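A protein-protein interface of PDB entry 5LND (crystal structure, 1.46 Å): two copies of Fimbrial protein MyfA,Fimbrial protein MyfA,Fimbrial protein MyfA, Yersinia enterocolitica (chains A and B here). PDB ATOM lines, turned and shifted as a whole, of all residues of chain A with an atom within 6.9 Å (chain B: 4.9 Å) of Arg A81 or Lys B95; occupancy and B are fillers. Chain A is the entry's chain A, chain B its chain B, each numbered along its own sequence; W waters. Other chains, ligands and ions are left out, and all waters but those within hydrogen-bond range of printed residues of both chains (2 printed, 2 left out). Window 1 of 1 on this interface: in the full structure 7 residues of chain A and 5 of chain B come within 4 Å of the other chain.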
ATOM      1  N   GLU A   5      -0.293  22.898   7.599  1.00  0.00           N
ATOM      2  CA  GLU A   5       0.718  23.910   7.875  1.00  0.00           C
ATOM      3  C   GLU A   5       1.342  23.631   9.238  1.00  0.00           C
ATOM      4  O   GLU A   5       0.643  23.465  10.226  1.00  0.00           O
ATOM      5  CB  GLU A   5       0.083  25.299   7.810  1.00  0.00           C
ATOM      6  CG  GLU A   5       0.640  26.345   8.750  1.00  0.00           C
ATOM      7  CD  GLU A   5      -0.319  27.520   8.903  1.00  0.00           C
ATOM      8  OE1 GLU A   5      -1.419  27.459   8.298  1.00  0.00           O
ATOM      9  OE2 GLU A   5       0.022  28.487   9.629  1.00  0.00           O
ATOM     10  N   HIS A  26       3.441  25.079  15.822  1.00  0.00           N
ATOM     11  CA  HIS A  26       2.032  25.298  15.548  1.00  0.00           C
ATOM     12  C   HIS A  26       1.564  24.535  14.310  1.00  0.00           C
ATOM     13  O   HIS A  26       2.262  24.485  13.289  1.00  0.00           O
ATOM     14  CB  HIS A  26       1.716  26.782  15.405  1.00  0.00           C
ATOM     15  CG  HIS A  26       0.251  27.063  15.296  1.00  0.00           C
ATOM     16  ND1 HIS A  26      -0.354  27.410  14.108  1.00  0.00           N
ATOM     17  CD2 HIS A  26      -0.738  27.004  16.218  1.00  0.00           C
ATOM     18  CE1 HIS A  26      -1.649  27.571  14.308  1.00  0.00           C
ATOM     19  NE2 HIS A  26      -1.908  27.330  15.579  1.00  0.00           N
ATOM     20  N   VAL A  28      -1.770  23.539  11.640  1.00  0.00           N
ATOM     21  CA  VAL A  28      -3.098  23.748  11.102  1.00  0.00           C
ATOM     22  C   VAL A  28      -3.435  22.686  10.068  1.00  0.00           C
ATOM     23  O   VAL A  28      -2.710  22.497   9.103  1.00  0.00           O
ATOM     24  CB  VAL A  28      -3.230  25.126  10.461  1.00  0.00           C
ATOM     25  CG1 VAL A  28      -4.652  25.316   9.959  1.00  0.00           C
ATOM     26  CG2 VAL A  28      -2.849  26.214  11.449  1.00  0.00           C
ATOM     27  N   MET A  29      -4.538  21.982  10.295  1.00  0.00           N
ATOM     28  CA  MET A  29      -5.000  20.932   9.396  1.00  0.00           C
ATOM     29  C   MET A  29      -6.379  21.319   8.892  1.00  0.00           C
ATOM     30  O   MET A  29      -7.303  21.528   9.677  1.00  0.00           O
ATOM     31  CB  MET A  29      -5.070  19.586  10.125  1.00  0.00           C
ATOM     32  CG  MET A  29      -3.726  19.050  10.605  1.00  0.00           C
ATOM     33  SD  MET A  29      -3.881  17.635  11.706  1.00  0.00           S
ATOM     34  CE  MET A  29      -4.755  18.342  13.079  1.00  0.00           C
ATOM     35  N   SER A  30      -6.516  21.440   7.580  1.00  0.00           N
ATOM     36  CA  SER A  30      -7.777  21.886   7.023  1.00  0.00           C
ATOM     37  C   SER A  30      -8.185  21.083   5.807  1.00  0.00           C
ATOM     38  O   SER A  30      -7.339  20.609   5.043  1.00  0.00           O
ATOM     39  CB  SER A  30      -7.719  23.367   6.678  1.00  0.00           C
ATOM     40  OG  SER A  30      -6.471  23.701   6.112  1.00  0.00           O
ATOM     41  N   ASP A  31      -9.490  20.896   5.667  1.00  0.00           N
ATOM     42  CA  ASP A  31     -10.052  20.278   4.488  1.00  0.00           C
ATOM     43  C   ASP A  31     -11.527  20.587   4.427  1.00  0.00           C
ATOM     44  O   ASP A  31     -12.238  20.452   5.416  1.00  0.00           O
ATOM     45  CB  ASP A  31      -9.847  18.769   4.470  1.00  0.00           C
ATOM     46  CG  ASP A  31     -10.178  18.177   3.122  1.00  0.00           C
ATOM     47  OD1 ASP A  31     -10.039  18.916   2.121  1.00  0.00           O
ATOM     48  OD2 ASP A  31     -10.593  17.002   3.048  1.00  0.00           O
ATOM     49  N   SER A  32     -11.980  20.999   3.249  1.00  0.00           N
ATOM     50  CA  SER A  32     -13.384  21.325   3.031  1.00  0.00           C
ATOM     51  C   SER A  32     -14.212  20.073   2.774  1.00  0.00           C
ATOM     52  O   SER A  32     -15.436  20.122   2.817  1.00  0.00           O
ATOM     53  CB  SER A  32     -13.520  22.247   1.837  1.00  0.00           C
ATOM     54  OG  SER A  32     -13.091  21.577   0.670  1.00  0.00           O
ATOM     55  N   HIS A  35     -15.158  14.707   6.558  1.00  0.00           N
ATOM     56  CA  HIS A  35     -14.185  13.914   7.327  1.00  0.00           C
ATOM     57  C   HIS A  35     -14.572  13.757   8.795  1.00  0.00           C
ATOM     58  O   HIS A  35     -15.405  14.507   9.297  1.00  0.00           O
ATOM     59  CB  HIS A  35     -12.765  14.490   7.194  1.00  0.00           C
ATOM     60  CG  HIS A  35     -12.590  15.851   7.795  1.00  0.00           C
ATOM     61  ND1 HIS A  35     -12.837  17.012   7.093  1.00  0.00           N
ATOM     62  CD2 HIS A  35     -12.163  16.242   9.020  1.00  0.00           C
ATOM     63  CE1 HIS A  35     -12.591  18.053   7.863  1.00  0.00           C
ATOM     64  NE2 HIS A  35     -12.180  17.613   9.039  1.00  0.00           N
ATOM     65  N   TRP A  38      -8.628  13.764  12.509  1.00  0.00           N
ATOM     66  CA  TRP A  38      -7.231  13.801  12.109  1.00  0.00           C
ATOM     67  C   TRP A  38      -6.332  13.009  13.056  1.00  0.00           C
ATOM     68  O   TRP A  38      -6.573  12.947  14.267  1.00  0.00           O
ATOM     69  CB  TRP A  38      -6.724  15.242  12.073  1.00  0.00           C
ATOM     70  CG  TRP A  38      -7.551  16.200  11.281  1.00  0.00           C
ATOM     71  CD1 TRP A  38      -8.624  16.901  11.723  1.00  0.00           C
ATOM     72  CD2 TRP A  38      -7.346  16.596   9.920  1.00  0.00           C
ATOM     73  NE1 TRP A  38      -9.114  17.700  10.723  1.00  0.00           N
ATOM     74  CE2 TRP A  38      -8.344  17.532   9.603  1.00  0.00           C
ATOM     75  CE3 TRP A  38      -6.419  16.247   8.932  1.00  0.00           C
ATOM     76  CZ2 TRP A  38      -8.446  18.119   8.343  1.00  0.00           C
ATOM     77  CZ3 TRP A  38      -6.524  16.833   7.681  1.00  0.00           C
ATOM     78  CH2 TRP A  38      -7.525  17.758   7.401  1.00  0.00           C
ATOM     79  N   ILE A  75      -7.732  13.575  16.876  1.00  0.00           N
ATOM     80  CA  ILE A  75      -8.907  14.348  17.244  1.00  0.00           C
ATOM     81  C   ILE A  75     -10.056  14.056  16.291  1.00  0.00           C
ATOM     82  O   ILE A  75      -9.849  13.885  15.087  1.00  0.00           O
ATOM     83  CB  ILE A  75      -8.588  15.859  17.286  1.00  0.00           C
ATOM     84  CG1 ILE A  75      -9.677  16.626  18.023  1.00  0.00           C
ATOM     85  CG2 ILE A  75      -8.382  16.434  15.886  1.00  0.00           C
ATOM     86  CD1 ILE A  75      -9.332  18.078  18.228  1.00  0.00           C
ATOM     87  N   ASP A  77     -12.923  15.845  14.644  1.00  0.00           N
ATOM     88  CA  ASP A  77     -13.263  17.221  14.354  1.00  0.00           C
ATOM     89  C   ASP A  77     -13.747  17.234  12.921  1.00  0.00           C
ATOM     90  O   ASP A  77     -12.971  16.978  11.994  1.00  0.00           O
ATOM     91  CB  ASP A  77     -12.030  18.114  14.532  1.00  0.00           C
ATOM     92  CG  ASP A  77     -12.336  19.594  14.376  1.00  0.00           C
ATOM     93  OD1 ASP A  77     -12.906  20.002  13.346  1.00  0.00           O
ATOM     94  OD2 ASP A  77     -11.973  20.363  15.284  1.00  0.00           O
ATOM     95  N   GLY A  78     -15.035  17.504  12.748  1.00  0.00           N
ATOM     96  CA  GLY A  78     -15.633  17.545  11.430  1.00  0.00           C
ATOM     97  C   GLY A  78     -15.588  18.899  10.749  1.00  0.00           C
ATOM     98  O   GLY A  78     -15.810  18.984   9.548  1.00  0.00           O
ATOM     99  N   SER A  79     -15.304  19.960  11.500  1.00  0.00           N
ATOM    100  CA  SER A  79     -15.224  21.286  10.901  1.00  0.00           C
ATOM    101  C   SER A  79     -14.122  21.323   9.845  1.00  0.00           C
ATOM    102  O   SER A  79     -13.335  20.381   9.720  1.00  0.00           O
ATOM    103  CB  SER A  79     -15.003  22.359  11.960  1.00  0.00           C
ATOM    104  OG  SER A  79     -13.650  22.461  12.328  1.00  0.00           O
ATOM    105  N   GLU A  80     -14.069  22.402   9.074  1.00  0.00           N
ATOM    106  CA  GLU A  80     -13.147  22.487   7.941  1.00  0.00           C
ATOM    107  C   GLU A  80     -11.685  22.634   8.387  1.00  0.00           C
ATOM    108  O   GLU A  80     -10.756  22.354   7.629  1.00  0.00           O
ATOM    109  CB  GLU A  80     -13.567  23.636   7.006  1.00  0.00           C
ATOM    110  CG  GLU A  80     -12.662  23.862   5.791  1.00  0.00           C
ATOM    111  CD  GLU A  80     -11.622  24.958   6.009  1.00  0.00           C
ATOM    112  OE1 GLU A  80     -11.824  25.789   6.909  1.00  0.00           O
ATOM    113  OE2 GLU A  80     -10.608  24.999   5.281  1.00  0.00           O
ATOM    114  N   ARG A  81     -11.489  23.035   9.636  1.00  0.00           N
ATOM    115  CA  ARG A  81     -10.174  23.465  10.086  1.00  0.00           C
ATOM    116  C   ARG A  81      -9.955  23.236  11.587  1.00  0.00           C
ATOM    117  O   ARG A  81     -10.841  23.482  12.400  1.00  0.00           O
ATOM    118  CB  ARG A  81     -10.018  24.943   9.738  1.00  0.00           C
ATOM    119  CG  ARG A  81      -8.669  25.532  10.025  1.00  0.00           C
ATOM    120  CD  ARG A  81      -8.628  26.939   9.503  1.00  0.00           C
ATOM    121  NE  ARG A  81      -7.345  27.596   9.712  1.00  0.00           N
ATOM    122  CZ  ARG A  81      -7.061  28.374  10.751  1.00  0.00           C
ATOM    123  NH1 ARG A  81      -7.964  28.595  11.693  1.00  0.00           N
ATOM    124  NH2 ARG A  81      -5.867  28.933  10.846  1.00  0.00           N
ATOM    125  N   VAL A  82      -8.774  22.754  11.952  1.00  0.00           N
ATOM    126  CA  VAL A  82      -8.447  22.556  13.362  1.00  0.00           C
ATOM    127  C   VAL A  82      -7.003  22.994  13.600  1.00  0.00           C
ATOM    128  O   VAL A  82      -6.125  22.718  12.781  1.00  0.00           O
ATOM    129  CB  VAL A  82      -8.677  21.096  13.800  1.00  0.00           C
ATOM    130  CG1 VAL A  82      -7.907  20.161  12.917  1.00  0.00           C
ATOM    131  CG2 VAL A  82      -8.288  20.889  15.245  1.00  0.00           C
ATOM    132  N   GLU A  83      -6.763  23.710  14.697  1.00  0.00           N
ATOM    133  CA  GLU A  83      -5.422  24.197  15.002  1.00  0.00           C
ATOM    134  C   GLU A  83      -4.886  23.643  16.309  1.00  0.00           C
ATOM    135  O   GLU A  83      -5.633  23.467  17.267  1.00  0.00           O
ATOM    136  CB  GLU A  83      -5.419  25.715  15.085  1.00  0.00           C
ATOM    137  CG  GLU A  83      -5.978  26.379  13.865  1.00  0.00           C
ATOM    138  CD  GLU A  83      -6.173  27.856  14.075  1.00  0.00           C
ATOM    139  OE1 GLU A  83      -7.214  28.236  14.660  1.00  0.00           O
ATOM    140  OE2 GLU A  83      -5.276  28.631  13.669  1.00  0.00           O
ATOM    141  N   SER B  15     -21.626  27.043  18.392  1.00  0.00           N
ATOM    142  CA  SER B  15     -20.690  26.047  17.873  1.00  0.00           C
ATOM    143  C   SER B  15     -21.170  24.620  18.105  1.00  0.00           C
ATOM    144  O   SER B  15     -21.922  24.356  19.042  1.00  0.00           O
ATOM    145  CB  SER B  15     -19.324  26.219  18.515  1.00  0.00           C
ATOM    146  OG  SER B  15     -19.431  26.196  19.920  1.00  0.00           O
ATOM    147  N   ASP B  55      -9.919  33.665  11.526  1.00  0.00           N
ATOM    148  CA  ASP B  55      -8.758  32.777  11.451  1.00  0.00           C
ATOM    149  C   ASP B  55      -8.752  31.947  10.179  1.00  0.00           C
ATOM    150  O   ASP B  55      -7.844  31.154   9.951  1.00  0.00           O
ATOM    151  CB  ASP B  55      -8.618  31.889  12.698  1.00  0.00           C
ATOM    152  CG  ASP B  55      -9.850  31.058  12.978  1.00  0.00           C
ATOM    153  OD1 ASP B  55     -10.732  30.988  12.109  1.00  0.00           O
ATOM    154  OD2 ASP B  55      -9.931  30.450  14.067  1.00  0.00           O
ATOM    155  N   GLY B  56      -9.775  32.128   9.355  1.00  0.00           N
ATOM    156  CA  GLY B  56      -9.818  31.474   8.063  1.00  0.00           C
ATOM    157  C   GLY B  56     -10.705  30.250   7.933  1.00  0.00           C
ATOM    158  O   GLY B  56     -10.802  29.679   6.856  1.00  0.00           O
ATOM    159  N   THR B  57     -11.342  29.836   9.018  1.00  0.00           N
ATOM    160  CA  THR B  57     -12.219  28.671   8.978  1.00  0.00           C
ATOM    161  C   THR B  57     -13.377  28.936   8.024  1.00  0.00           C
ATOM    162  O   THR B  57     -13.985  30.002   8.073  1.00  0.00           O
ATOM    163  CB  THR B  57     -12.793  28.336  10.372  1.00  0.00           C
ATOM    164  OG1 THR B  57     -11.730  28.263  11.326  1.00  0.00           O
ATOM    165  CG2 THR B  57     -13.509  27.002  10.353  1.00  0.00           C
ATOM    166  N   GLU B  93     -20.322  20.581  11.429  1.00  0.00           N
ATOM    167  CA  GLU B  93     -19.674  20.891  12.688  1.00  0.00           C
ATOM    168  C   GLU B  93     -19.046  22.259  12.572  1.00  0.00           C
ATOM    169  O   GLU B  93     -18.062  22.435  11.865  1.00  0.00           O
ATOM    170  CB  GLU B  93     -18.625  19.841  13.021  1.00  0.00           C
ATOM    171  CG  GLU B  93     -19.225  18.453  13.180  1.00  0.00           C
ATOM    172  CD  GLU B  93     -18.453  17.599  14.166  1.00  0.00           C
ATOM    173  OE1 GLU B  93     -17.364  18.046  14.600  1.00  0.00           O
ATOM    174  OE2 GLU B  93     -18.939  16.493  14.503  1.00  0.00           O
ATOM    175  N   VAL B  94     -19.636  23.232  13.256  1.00  0.00           N
ATOM    176  CA  VAL B  94     -19.256  24.628  13.099  1.00  0.00           C
ATOM    177  C   VAL B  94     -18.609  25.174  14.353  1.00  0.00           C
ATOM    178  O   VAL B  94     -19.127  25.015  15.447  1.00  0.00           O
ATOM    179  CB  VAL B  94     -20.469  25.487  12.774  1.00  0.00           C
ATOM    180  CG1 VAL B  94     -20.058  26.926  12.651  1.00  0.00           C
ATOM    181  CG2 VAL B  94     -21.115  25.019  11.483  1.00  0.00           C
ATOM    182  N   LYS B  95     -17.475  25.832  14.181  1.00  0.00           N
ATOM    183  CA  LYS B  95     -16.761  26.414  15.293  1.00  0.00           C
ATOM    184  C   LYS B  95     -17.187  27.856  15.479  1.00  0.00           C
ATOM    185  O   LYS B  95     -17.734  28.467  14.571  1.00  0.00           O
ATOM    186  CB  LYS B  95     -15.267  26.347  15.024  1.00  0.00           C
ATOM    187  CG  LYS B  95     -14.773  24.946  14.781  1.00  0.00           C
ATOM    188  CD  LYS B  95     -13.273  24.832  15.005  1.00  0.00           C
ATOM    189  CE  LYS B  95     -12.894  23.436  15.487  1.00  0.00           C
ATOM    190  NZ  LYS B  95     -11.658  22.894  14.843  1.00  0.00           N
ATOM    191  N   ALA B  96     -16.930  28.395  16.665  1.00  0.00           N
ATOM    192  CA  ALA B  96     -17.264  29.780  16.960  1.00  0.00           C
ATOM    193  C   ALA B  96     -16.465  30.716  16.067  1.00  0.00           C
ATOM    194  O   ALA B  96     -15.359  30.385  15.648  1.00  0.00           O
ATOM    195  CB  ALA B  96     -17.004  30.089  18.429  1.00  0.00           C
ATOM    196  N   GLY B  97     -17.029  31.881  15.771  1.00  0.00           N
ATOM    197  CA  GLY B  97     -16.324  32.876  14.986  1.00  0.00           C
ATOM    198  C   GLY B  97     -17.225  33.928  14.380  1.00  0.00           C
ATOM    199  O   GLY B  97     -18.448  33.826  14.436  1.00  0.00           O
ATOM    200  N   TYR B  99     -18.127  35.059  10.947  1.00  0.00           N
ATOM    201  CA  TYR B  99     -17.923  34.582   9.592  1.00  0.00           C
ATOM    202  C   TYR B  99     -18.463  35.536   8.554  1.00  0.00           C
ATOM    203  O   TYR B  99     -19.648  35.853   8.545  1.00  0.00           O
ATOM    204  CB  TYR B  99     -18.586  33.239   9.402  1.00  0.00           C
ATOM    205  CG  TYR B  99     -18.014  32.091  10.177  1.00  0.00           C
ATOM    206  CD1 TYR B  99     -17.100  31.234   9.588  1.00  0.00           C
ATOM    207  CD2 TYR B  99     -18.432  31.824  11.473  1.00  0.00           C
ATOM    208  CE1 TYR B  99     -16.597  30.159  10.269  1.00  0.00           C
ATOM    209  CE2 TYR B  99     -17.930  30.746  12.167  1.00  0.00           C
ATOM    210  CZ  TYR B  99     -17.011  29.925  11.558  1.00  0.00           C
ATOM    211  OH  TYR B  99     -16.505  28.846  12.231  1.00  0.00           O
ATOM    212  N   VAL B 130     -21.005  33.016  15.067  1.00  0.00           N
ATOM    213  CA  VAL B 130     -21.225  31.705  15.655  1.00  0.00           C
ATOM    214  C   VAL B 130     -20.685  31.766  17.075  1.00  0.00           C
ATOM    215  O   VAL B 130     -19.501  32.019  17.287  1.00  0.00           O
ATOM    216  CB  VAL B 130     -20.541  30.578  14.867  1.00  0.00           C
ATOM    217  CG1 VAL B 130     -20.567  29.299  15.667  1.00  0.00           C
ATOM    218  CG2 VAL B 130     -21.236  30.368  13.538  1.00  0.00           C
HETATM  219  O   HOH W   1      -9.241  24.272  15.823  1.00  0.00           O
HETATM  220  O   HOH W   2     -18.242  19.872   9.036  1.00  0.00           O
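NZ of Lys B95 lies within salt-bridge range of OD2 of Asp A77 (2.6 Å). The side-chain carboxylate of Glu B93 lies within hydrogen-bond range of the backbone NH of Gly A78 (3.0 Å). OG of Ser A79 lies within hydrogen-bond range of NZ of Lys B95. OD2 of Asp B55 is in salt-bridge range of NH1 of Arg A81, at 3.6 Å. O of Arg A81 sits at hydrogen-bond distance from NZ of Lys B95 (2.6 Å).
The backbone carbonyl oxygen (O) of Met A29 is in hydrogen-bond range of the backbone NH (N) of Val A82 (3.0 Å). A ring nitrogen (NE2) of His A35 is in hydrogen-bond range of the backbone carbonyl oxygen (O) of Asp A77, at 3.1 Å. A ring nitrogen (NE2) of His A35 sits close to the backbone carbonyl oxygen (O) of Ser A79 (3.1 Å). OD1 of Asp A77 lies within hydrogen-bond range of OG of Ser A79 (2.8 Å). The backbone carbonyl oxygen (O) of Arg A81 lies within hydrogen-bond range of the side-chain hydroxyl (OG) of Ser A79. The guanidinium group (NH2) of Arg A81 is in salt-bridge range of the side-chain carboxylate (OE2) of Glu A83 (2.9 Å).
Among the printed residues, pairs that only touch across the chains: Ser A79 with Glu B93 (3.1 Å), Val A82 with Lys B95 (3.6 Å), Glu A83 with Asp B55 (3.6 Å), Glu A80 with Thr B57 (3.6 Å) and Arg A81 with Thr B57 (3.8 Å).
Ser A32 touches none of the printed residues of chain B. Of the printed residues of chain B, Asp A77 touches Lys B95. Of the printed residues of chain B, Glu A80 touches Thr B57. Of the printed residues of chain B, Glu A83 touches Asp B55. Printed residues of chain A within 4 Å of Thr B57: Glu A80 (3.6 Å) and Arg A81 (3.8 Å). Printed residues of chain A within 4 Å of Glu B93: Gly A78 and Ser A79. Of the printed residues of chain A, Lys B95 touches Asp A77, Ser A79, Arg A81 and Val A82. Val B130 touches none of the printed residues of chain A. The nearest residue of chain B that does not touch Arg A81 is Gly B56 (4.2 Å). The nearest residue of chain A that does not touch Lys B95 is Glu A83 (5.0 Å).
Of the 17 printed residues of chain A, 7 touch a printed residue of chain B. Along chain A the printed residues that touch a printed residue of chain B span positions 77 to 83. Of the 11 printed residues of chain B, 4 touch a printed residue of chain A. Along chain B the printed residues that touch a printed residue of chain A span positions 55 to 95.
No position is printed for both chains. Of the 10 pairs that touch across the chains among the printed residues, none has its exchanged pair printed and touching as well.
Water W2 lies within hydrogen-bond range of O of Gly A78 and N of Glu B93. Water W1 lies within hydrogen-bond range of N of Glu A83 and NZ of Lys B95.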
